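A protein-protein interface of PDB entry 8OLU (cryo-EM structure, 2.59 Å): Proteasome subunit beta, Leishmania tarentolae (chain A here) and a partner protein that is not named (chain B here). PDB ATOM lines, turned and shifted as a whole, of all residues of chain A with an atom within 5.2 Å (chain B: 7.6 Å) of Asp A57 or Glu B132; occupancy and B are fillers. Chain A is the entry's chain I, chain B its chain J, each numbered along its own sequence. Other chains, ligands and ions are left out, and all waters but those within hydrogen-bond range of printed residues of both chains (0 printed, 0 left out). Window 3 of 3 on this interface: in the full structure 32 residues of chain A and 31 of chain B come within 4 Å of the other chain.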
ATOM      1  N   THR A  47      -5.497  -2.432  13.804  1.00  0.00           N
ATOM      2  CA  THR A  47      -5.408  -3.717  13.157  1.00  0.00           C
ATOM      3  C   THR A  47      -4.207  -4.531  13.588  1.00  0.00           C
ATOM      4  O   THR A  47      -3.979  -5.569  13.050  1.00  0.00           O
ATOM      5  CB  THR A  47      -5.333  -3.549  11.651  1.00  0.00           C
ATOM      6  OG1 THR A  47      -4.058  -2.972  11.327  1.00  0.00           O
ATOM      7  CG2 THR A  47      -6.473  -2.711  11.114  1.00  0.00           C
ATOM      8  N   ARG A  48      -3.504  -4.198  14.619  1.00  0.00           N
ATOM      9  CA  ARG A  48      -2.415  -5.087  14.951  1.00  0.00           C
ATOM     10  C   ARG A  48      -2.898  -6.237  15.806  1.00  0.00           C
ATOM     11  O   ARG A  48      -3.276  -6.036  16.951  1.00  0.00           O
ATOM     12  CB  ARG A  48      -1.392  -4.276  15.737  1.00  0.00           C
ATOM     13  CG  ARG A  48      -0.298  -5.068  16.414  1.00  0.00           C
ATOM     14  CD  ARG A  48       0.533  -4.123  17.279  1.00  0.00           C
ATOM     15  NE  ARG A  48       1.288  -3.326  16.351  1.00  0.00           N
ATOM     16  CZ  ARG A  48       2.161  -2.412  16.718  1.00  0.00           C
ATOM     17  NH1 ARG A  48       2.506  -2.226  17.991  1.00  0.00           N
ATOM     18  NH2 ARG A  48       2.679  -1.682  15.755  1.00  0.00           N
ATOM     19  N   ALA A  49      -2.740  -7.454  15.312  1.00  0.00           N
ATOM     20  CA  ALA A  49      -2.889  -8.640  16.151  1.00  0.00           C
ATOM     21  C   ALA A  49      -1.526  -9.071  16.664  1.00  0.00           C
ATOM     22  O   ALA A  49      -0.756  -9.619  15.894  1.00  0.00           O
ATOM     23  CB  ALA A  49      -3.496  -9.755  15.345  1.00  0.00           C
ATOM     24  N   THR A  50      -1.264  -8.848  17.953  1.00  0.00           N
ATOM     25  CA  THR A  50      -0.089  -9.407  18.582  1.00  0.00           C
ATOM     26  C   THR A  50      -0.318 -10.856  18.997  1.00  0.00           C
ATOM     27  O   THR A  50      -1.437 -11.382  18.982  1.00  0.00           O
ATOM     28  CB  THR A  50       0.358  -8.657  19.849  1.00  0.00           C
ATOM     29  OG1 THR A  50      -0.624  -8.808  20.886  1.00  0.00           O
ATOM     30  CG2 THR A  50       0.656  -7.201  19.589  1.00  0.00           C
ATOM     31  N   VAL A  55       4.138  -8.901  16.631  1.00  0.00           N
ATOM     32  CA  VAL A  55       3.022  -8.665  15.757  1.00  0.00           C
ATOM     33  C   VAL A  55       2.826  -9.814  14.786  1.00  0.00           C
ATOM     34  O   VAL A  55       3.463  -9.903  13.736  1.00  0.00           O
ATOM     35  CB  VAL A  55       3.307  -7.344  15.033  1.00  0.00           C
ATOM     36  CG1 VAL A  55       2.246  -7.012  14.034  1.00  0.00           C
ATOM     37  CG2 VAL A  55       3.504  -6.225  16.050  1.00  0.00           C
ATOM     38  N   ALA A  56       1.908 -10.709  15.110  1.00  0.00           N
ATOM     39  CA  ALA A  56       1.649 -11.853  14.249  1.00  0.00           C
ATOM     40  C   ALA A  56       1.060 -11.392  12.948  1.00  0.00           C
ATOM     41  O   ALA A  56       1.328 -11.984  11.925  1.00  0.00           O
ATOM     42  CB  ALA A  56       0.674 -12.789  14.901  1.00  0.00           C
ATOM     43  N   ASP A  57       0.145 -10.431  13.022  1.00  0.00           N
ATOM     44  CA  ASP A  57      -0.528  -9.942  11.832  1.00  0.00           C
ATOM     45  C   ASP A  57      -0.626  -8.440  11.958  1.00  0.00           C
ATOM     46  O   ASP A  57      -1.124  -7.930  12.933  1.00  0.00           O
ATOM     47  CB  ASP A  57      -1.928 -10.529  11.604  1.00  0.00           C
ATOM     48  CG  ASP A  57      -2.552 -10.137  10.260  1.00  0.00           C
ATOM     49  OD1 ASP A  57      -1.868  -9.385   9.483  1.00  0.00           O
ATOM     50  OD2 ASP A  57      -3.715 -10.610   9.962  1.00  0.00           O
ATOM     51  N   LYS A  58      -0.194  -7.776  10.912  1.00  0.00           N
ATOM     52  CA  LYS A  58      -0.169  -6.342  10.906  1.00  0.00           C
ATOM     53  C   LYS A  58      -1.565  -5.848  10.606  1.00  0.00           C
ATOM     54  O   LYS A  58      -1.913  -4.792  11.107  1.00  0.00           O
ATOM     55  CB  LYS A  58       0.908  -5.871   9.934  1.00  0.00           C
ATOM     56  CG  LYS A  58       2.278  -5.767  10.598  1.00  0.00           C
ATOM     57  CD  LYS A  58       3.439  -5.411   9.682  1.00  0.00           C
ATOM     58  CE  LYS A  58       3.726  -6.489   8.655  1.00  0.00           C
ATOM     59  NZ  LYS A  58       5.108  -6.360   8.145  1.00  0.00           N
ATOM     60  N   ARG A  59      -2.370  -6.618   9.874  1.00  0.00           N
ATOM     61  CA  ARG A  59      -3.587  -6.086   9.299  1.00  0.00           C
ATOM     62  C   ARG A  59      -4.787  -6.983   9.548  1.00  0.00           C
ATOM     63  O   ARG A  59      -5.545  -7.228   8.612  1.00  0.00           O
ATOM     64  CB  ARG A  59      -3.447  -5.896   7.790  1.00  0.00           C
ATOM     65  CG  ARG A  59      -2.810  -4.563   7.426  1.00  0.00           C
ATOM     66  CD  ARG A  59      -2.764  -4.254   5.930  1.00  0.00           C
ATOM     67  NE  ARG A  59      -1.830  -5.128   5.226  1.00  0.00           N
ATOM     68  CZ  ARG A  59      -0.501  -5.083   5.350  1.00  0.00           C
ATOM     69  NH1 ARG A  59       0.226  -6.127   4.981  1.00  0.00           N
ATOM     70  NH2 ARG A  59       0.090  -4.002   5.841  1.00  0.00           N
ATOM     71  N   CYS A  60      -5.053  -7.385  10.798  1.00  0.00           N
ATOM     72  CA  CYS A  60      -6.263  -8.164  10.998  1.00  0.00           C
ATOM     73  C   CYS A  60      -7.495  -7.268  11.123  1.00  0.00           C
ATOM     74  O   CYS A  60      -7.370  -6.112  11.497  1.00  0.00           O
ATOM     75  CB  CYS A  60      -6.209  -9.091  12.192  1.00  0.00           C
ATOM     76  SG  CYS A  60      -6.057  -8.153  13.710  1.00  0.00           S
ATOM     77  N   GLY B  84      -9.167 -24.986   2.468  1.00  0.00           N
ATOM     78  CA  GLY B  84      -8.389 -24.520   3.582  1.00  0.00           C
ATOM     79  C   GLY B  84      -9.177 -23.614   4.507  1.00  0.00           C
ATOM     80  O   GLY B  84      -8.889 -23.535   5.697  1.00  0.00           O
ATOM     81  N   LYS B  85     -10.170 -22.913   3.976  1.00  0.00           N
ATOM     82  CA  LYS B  85     -10.899 -22.030   4.866  1.00  0.00           C
ATOM     83  C   LYS B  85     -11.773 -22.851   5.788  1.00  0.00           C
ATOM     84  O   LYS B  85     -11.763 -22.679   6.993  1.00  0.00           O
ATOM     85  CB  LYS B  85     -11.606 -20.966   4.032  1.00  0.00           C
ATOM     86  CG  LYS B  85     -10.858 -19.635   3.989  1.00  0.00           C
ATOM     87  CD  LYS B  85     -10.863 -18.952   2.617  1.00  0.00           C
ATOM     88  CE  LYS B  85     -10.700 -17.446   2.721  1.00  0.00           C
ATOM     89  NZ  LYS B  85      -9.912 -16.916   1.584  1.00  0.00           N
ATOM     90  N   ALA B  88      -9.665 -24.630   8.275  1.00  0.00           N
ATOM     91  CA  ALA B  88      -9.127 -23.875   9.372  1.00  0.00           C
ATOM     92  C   ALA B  88     -10.200 -23.476  10.350  1.00  0.00           C
ATOM     93  O   ALA B  88      -9.956 -23.319  11.502  1.00  0.00           O
ATOM     94  CB  ALA B  88      -8.493 -22.635   8.833  1.00  0.00           C
ATOM     95  N   ALA B  89     -11.367 -23.139   9.832  1.00  0.00           N
ATOM     96  CA  ALA B  89     -12.543 -22.937  10.648  1.00  0.00           C
ATOM     97  C   ALA B  89     -12.811 -24.160  11.484  1.00  0.00           C
ATOM     98  O   ALA B  89     -13.104 -24.045  12.641  1.00  0.00           O
ATOM     99  CB  ALA B  89     -13.676 -22.702   9.732  1.00  0.00           C
ATOM    100  N   TYR B 120      -4.048 -19.360   1.348  1.00  0.00           N
ATOM    101  CA  TYR B 120      -4.637 -19.056   2.609  1.00  0.00           C
ATOM    102  C   TYR B 120      -3.713 -19.649   3.621  1.00  0.00           C
ATOM    103  O   TYR B 120      -3.351 -20.803   3.504  1.00  0.00           O
ATOM    104  CB  TYR B 120      -6.047 -19.632   2.613  1.00  0.00           C
ATOM    105  CG  TYR B 120      -6.727 -19.419   3.926  1.00  0.00           C
ATOM    106  CD1 TYR B 120      -7.073 -18.141   4.348  1.00  0.00           C
ATOM    107  CD2 TYR B 120      -6.907 -20.479   4.787  1.00  0.00           C
ATOM    108  CE1 TYR B 120      -7.594 -17.929   5.615  1.00  0.00           C
ATOM    109  CE2 TYR B 120      -7.446 -20.285   6.050  1.00  0.00           C
ATOM    110  CZ  TYR B 120      -7.800 -19.013   6.463  1.00  0.00           C
ATOM    111  OH  TYR B 120      -8.336 -18.907   7.719  1.00  0.00           O
ATOM    112  N   LEU B 121      -3.229 -18.842   4.510  1.00  0.00           N
ATOM    113  CA  LEU B 121      -2.478 -19.364   5.602  1.00  0.00           C
ATOM    114  C   LEU B 121      -3.253 -19.071   6.857  1.00  0.00           C
ATOM    115  O   LEU B 121      -3.915 -18.053   6.946  1.00  0.00           O
ATOM    116  CB  LEU B 121      -1.217 -18.541   5.735  1.00  0.00           C
ATOM    117  CG  LEU B 121      -0.346 -18.461   4.489  1.00  0.00           C
ATOM    118  CD1 LEU B 121       0.854 -17.629   4.834  1.00  0.00           C
ATOM    119  CD2 LEU B 121       0.058 -19.829   4.016  1.00  0.00           C
ATOM    120  N   CYS B 122      -3.053 -19.843   7.888  1.00  0.00           N
ATOM    121  CA  CYS B 122      -3.738 -19.549   9.102  1.00  0.00           C
ATOM    122  C   CYS B 122      -2.942 -20.220  10.146  1.00  0.00           C
ATOM    123  O   CYS B 122      -2.554 -21.303   9.873  1.00  0.00           O
ATOM    124  CB  CYS B 122      -5.121 -20.167   9.092  1.00  0.00           C
ATOM    125  SG  CYS B 122      -6.025 -19.801  10.621  1.00  0.00           S
ATOM    126  N   ALA B 123      -2.596 -19.536  11.198  1.00  0.00           N
ATOM    127  CA  ALA B 123      -2.018 -20.155  12.358  1.00  0.00           C
ATOM    128  C   ALA B 123      -3.005 -19.846  13.435  1.00  0.00           C
ATOM    129  O   ALA B 123      -3.812 -18.973  13.225  1.00  0.00           O
ATOM    130  CB  ALA B 123      -0.687 -19.582  12.715  1.00  0.00           C
ATOM    131  N   THR B 124      -3.013 -20.631  14.497  1.00  0.00           N
ATOM    132  CA  THR B 124      -3.907 -20.373  15.606  1.00  0.00           C
ATOM    133  C   THR B 124      -3.132 -20.536  16.912  1.00  0.00           C
ATOM    134  O   THR B 124      -2.199 -21.325  16.987  1.00  0.00           O
ATOM    135  CB  THR B 124      -5.163 -21.278  15.563  1.00  0.00           C
ATOM    136  OG1 THR B 124      -4.758 -22.561  16.031  1.00  0.00           O
ATOM    137  CG2 THR B 124      -5.870 -21.460  14.217  1.00  0.00           C
ATOM    138  N   ALA B 129      -7.890 -19.047  18.249  1.00  0.00           N
ATOM    139  CA  ALA B 129      -7.828 -17.733  17.639  1.00  0.00           C
ATOM    140  C   ALA B 129      -7.020 -17.753  16.362  1.00  0.00           C
ATOM    141  O   ALA B 129      -5.799 -17.792  16.426  1.00  0.00           O
ATOM    142  CB  ALA B 129      -7.161 -16.748  18.567  1.00  0.00           C
ATOM    143  N   PRO B 130      -7.633 -17.507  15.199  1.00  0.00           N
ATOM    144  CA  PRO B 130      -6.885 -17.475  13.956  1.00  0.00           C
ATOM    145  C   PRO B 130      -6.085 -16.193  13.745  1.00  0.00           C
ATOM    146  O   PRO B 130      -6.262 -15.170  14.393  1.00  0.00           O
ATOM    147  CB  PRO B 130      -7.968 -17.623  12.902  1.00  0.00           C
ATOM    148  CG  PRO B 130      -9.101 -16.853  13.528  1.00  0.00           C
ATOM    149  CD  PRO B 130      -9.040 -17.166  15.011  1.00  0.00           C
ATOM    150  N   CYS B 131      -5.149 -16.334  12.829  1.00  0.00           N
ATOM    151  CA  CYS B 131      -4.201 -15.333  12.429  1.00  0.00           C
ATOM    152  C   CYS B 131      -4.083 -15.577  10.941  1.00  0.00           C
ATOM    153  O   CYS B 131      -3.560 -16.604  10.571  1.00  0.00           O
ATOM    154  CB  CYS B 131      -2.894 -15.588  13.166  1.00  0.00           C
ATOM    155  SG  CYS B 131      -1.565 -14.426  12.782  1.00  0.00           S
ATOM    156  N   GLU B 132      -4.724 -14.774  10.104  1.00  0.00           N
ATOM    157  CA  GLU B 132      -4.758 -15.092   8.700  1.00  0.00           C
ATOM    158  C   GLU B 132      -4.014 -13.996   7.957  1.00  0.00           C
ATOM    159  O   GLU B 132      -4.604 -13.190   7.247  1.00  0.00           O
ATOM    160  CB  GLU B 132      -6.180 -15.221   8.159  1.00  0.00           C
ATOM    161  CG  GLU B 132      -7.152 -16.047   8.992  1.00  0.00           C
ATOM    162  CD  GLU B 132      -8.646 -15.745   8.724  1.00  0.00           C
ATOM    163  OE1 GLU B 132      -9.119 -14.649   9.183  1.00  0.00           O
ATOM    164  OE2 GLU B 132      -9.362 -16.581   8.036  1.00  0.00           O
ATOM    165  N   PRO B 133      -2.684 -13.954   8.009  1.00  0.00           N
ATOM    166  CA  PRO B 133      -1.918 -12.964   7.296  1.00  0.00           C
ATOM    167  C   PRO B 133      -1.678 -13.457   5.908  1.00  0.00           C
ATOM    168  O   PRO B 133      -2.060 -14.573   5.576  1.00  0.00           O
ATOM    169  CB  PRO B 133      -0.606 -12.917   8.043  1.00  0.00           C
ATOM    170  CG  PRO B 133      -0.800 -13.799   9.243  1.00  0.00           C
ATOM    171  CD  PRO B 133      -1.769 -14.835   8.703  1.00  0.00           C
ATOM    172  N   GLU B 134      -1.125 -12.557   5.121  1.00  0.00           N
ATOM    173  CA  GLU B 134      -0.983 -12.722   3.683  1.00  0.00           C
ATOM    174  C   GLU B 134       0.429 -13.253   3.360  1.00  0.00           C
ATOM    175  O   GLU B 134       0.679 -13.716   2.241  1.00  0.00           O
ATOM    176  CB  GLU B 134      -1.203 -11.341   3.057  1.00  0.00           C
ATOM    177  CG  GLU B 134      -0.032 -10.391   3.398  1.00  0.00           C
ATOM    178  CD  GLU B 134       0.165  -9.107   2.605  1.00  0.00           C
ATOM    179  OE1 GLU B 134      -0.628  -8.855   1.653  1.00  0.00           O
ATOM    180  OE2 GLU B 134       1.110  -8.349   2.962  1.00  0.00           O
ATOM    181  N   ASP B 135       1.343 -13.114   4.351  1.00  0.00           N
ATOM    182  CA  ASP B 135       2.772 -13.308   4.146  1.00  0.00           C
ATOM    183  C   ASP B 135       3.232 -14.692   4.613  1.00  0.00           C
ATOM    184  O   ASP B 135       3.474 -15.603   3.807  1.00  0.00           O
ATOM    185  CB  ASP B 135       3.622 -12.215   4.802  1.00  0.00           C
ATOM    186  CG  ASP B 135       3.203 -11.671   6.155  1.00  0.00           C
ATOM    187  OD1 ASP B 135       2.329 -12.238   6.763  1.00  0.00           O
ATOM    188  OD2 ASP B 135       3.777 -10.636   6.580  1.00  0.00           O
ATOM    189  N   TYR B 136       3.188 -14.874   5.923  1.00  0.00           N
ATOM    190  CA  TYR B 136       3.771 -16.031   6.512  1.00  0.00           C
ATOM    191  C   TYR B 136       3.247 -16.151   7.926  1.00  0.00           C
ATOM    192  O   TYR B 136       2.914 -15.164   8.543  1.00  0.00           O
ATOM    193  CB  TYR B 136       5.258 -15.758   6.397  1.00  0.00           C
ATOM    194  CG  TYR B 136       5.740 -14.727   7.367  1.00  0.00           C
ATOM    195  CD1 TYR B 136       5.806 -15.099   8.686  1.00  0.00           C
ATOM    196  CD2 TYR B 136       6.055 -13.415   7.010  1.00  0.00           C
ATOM    197  CE1 TYR B 136       6.186 -14.206   9.669  1.00  0.00           C
ATOM    198  CE2 TYR B 136       6.444 -12.495   7.979  1.00  0.00           C
ATOM    199  CZ  TYR B 136       6.518 -12.910   9.318  1.00  0.00           C
ATOM    200  OH  TYR B 136       6.907 -12.215  10.471  1.00  0.00           O
ATOM    201  N   VAL B 137       3.144 -17.352   8.444  1.00  0.00           N
ATOM    202  CA  VAL B 137       2.662 -17.566   9.795  1.00  0.00           C
ATOM    203  C   VAL B 137       3.670 -18.463  10.419  1.00  0.00           C
ATOM    204  O   VAL B 137       4.348 -19.125   9.680  1.00  0.00           O
ATOM    205  CB  VAL B 137       1.307 -18.283   9.856  1.00  0.00           C
ATOM    206  CG1 VAL B 137       0.165 -17.376   9.489  1.00  0.00           C
ATOM    207  CG2 VAL B 137       1.220 -19.505   8.939  1.00  0.00           C
ATOM    208  N   HIS B 147       9.836 -15.130  12.840  1.00  0.00           N
ATOM    209  CA  HIS B 147       9.263 -13.835  12.535  1.00  0.00           C
ATOM    210  C   HIS B 147      10.384 -12.888  12.148  1.00  0.00           C
ATOM    211  O   HIS B 147      10.294 -12.164  11.171  1.00  0.00           O
ATOM    212  CB  HIS B 147       8.505 -13.290  13.760  1.00  0.00           C
ATOM    213  CG  HIS B 147       7.126 -13.823  13.900  1.00  0.00           C
ATOM    214  ND1 HIS B 147       6.189 -13.728  12.875  1.00  0.00           N
ATOM    215  CD2 HIS B 147       6.582 -14.535  14.940  1.00  0.00           C
ATOM    216  CE1 HIS B 147       5.079 -14.369  13.273  1.00  0.00           C
ATOM    217  NE2 HIS B 147       5.303 -14.879  14.564  1.00  0.00           N
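OE2 of Glu B134 is in salt-bridge range of NH1 of Arg A59 (3.1 Å).
N of Ala A56 sits at hydrogen-bond distance from O of Ala A49 (3.0 Å).
The backbone carbonyl oxygen (O) of Asp A57 sits at hydrogen-bond distance from the backbone NH (N) of Ala A49.
The side-chain carboxylate (OD1) of Asp A57 lies within hydrogen-bond range of the backbone NH (N) of Arg A59, at 2.8 Å.
N of Cys B131 lies within hydrogen-bond range of O of Ala B123 (3.0 Å).
OE2 of Glu B132 lies within hydrogen-bond range of OH of Tyr B120 (2.6 Å).
Cys B131 touches Ala A56.
Ala A56 touches Pro B133 (O to CG, 3.9 Å).
Asp A57 touches Glu B132 (OD2 to O, 3.8 Å).
Asp A57 touches Pro B133.
Of the printed residues of chain B, Asp A57 touches Glu B132 (3.8 Å) and Pro B133 (3.98 Å).
Of chain A, only Asp A57 (3.8 Å) comes within 4 Å of Glu B132.
Ala A56 touches just these residues of chain B: Cys B131 (3.5 Å) and Pro B133 (3.9 Å).
Of the printed residues of chain B, Arg A59 touches Glu B134 (3.1 Å).
Of the printed residues of chain A, Glu B134 touches Arg A59.
Of the printed residues of chain A, Cys B131 touches Ala A56 (3.5 Å).
Printed residues of chain A within 4 Å of Pro B133: Ala A56 and Asp A57.
His B147 touches none of the printed residues of chain A.
Tyr B136 touches none of the printed residues of chain A.
The nearest printed residue of chain B that does not touch Asp A57 is Cys B131 (4.1 Å).
The nearest printed residue of chain A that does not touch Glu B132 is Arg A59 (6.2 Å).
Of the 10 printed residues of chain A, 3 touch a printed residue of chain B.
Hydrophobic or aromatic side chains of chain A that line the printed part of chain B: Ala A56.
Of the 19 printed residues of chain B, 4 touch a printed residue of chain A.
Among the printed residues, Asp or Glu carboxylates within 4 Å of a Lys or Arg side-chain nitrogen of the other chain: Arg A59 with Glu B134.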
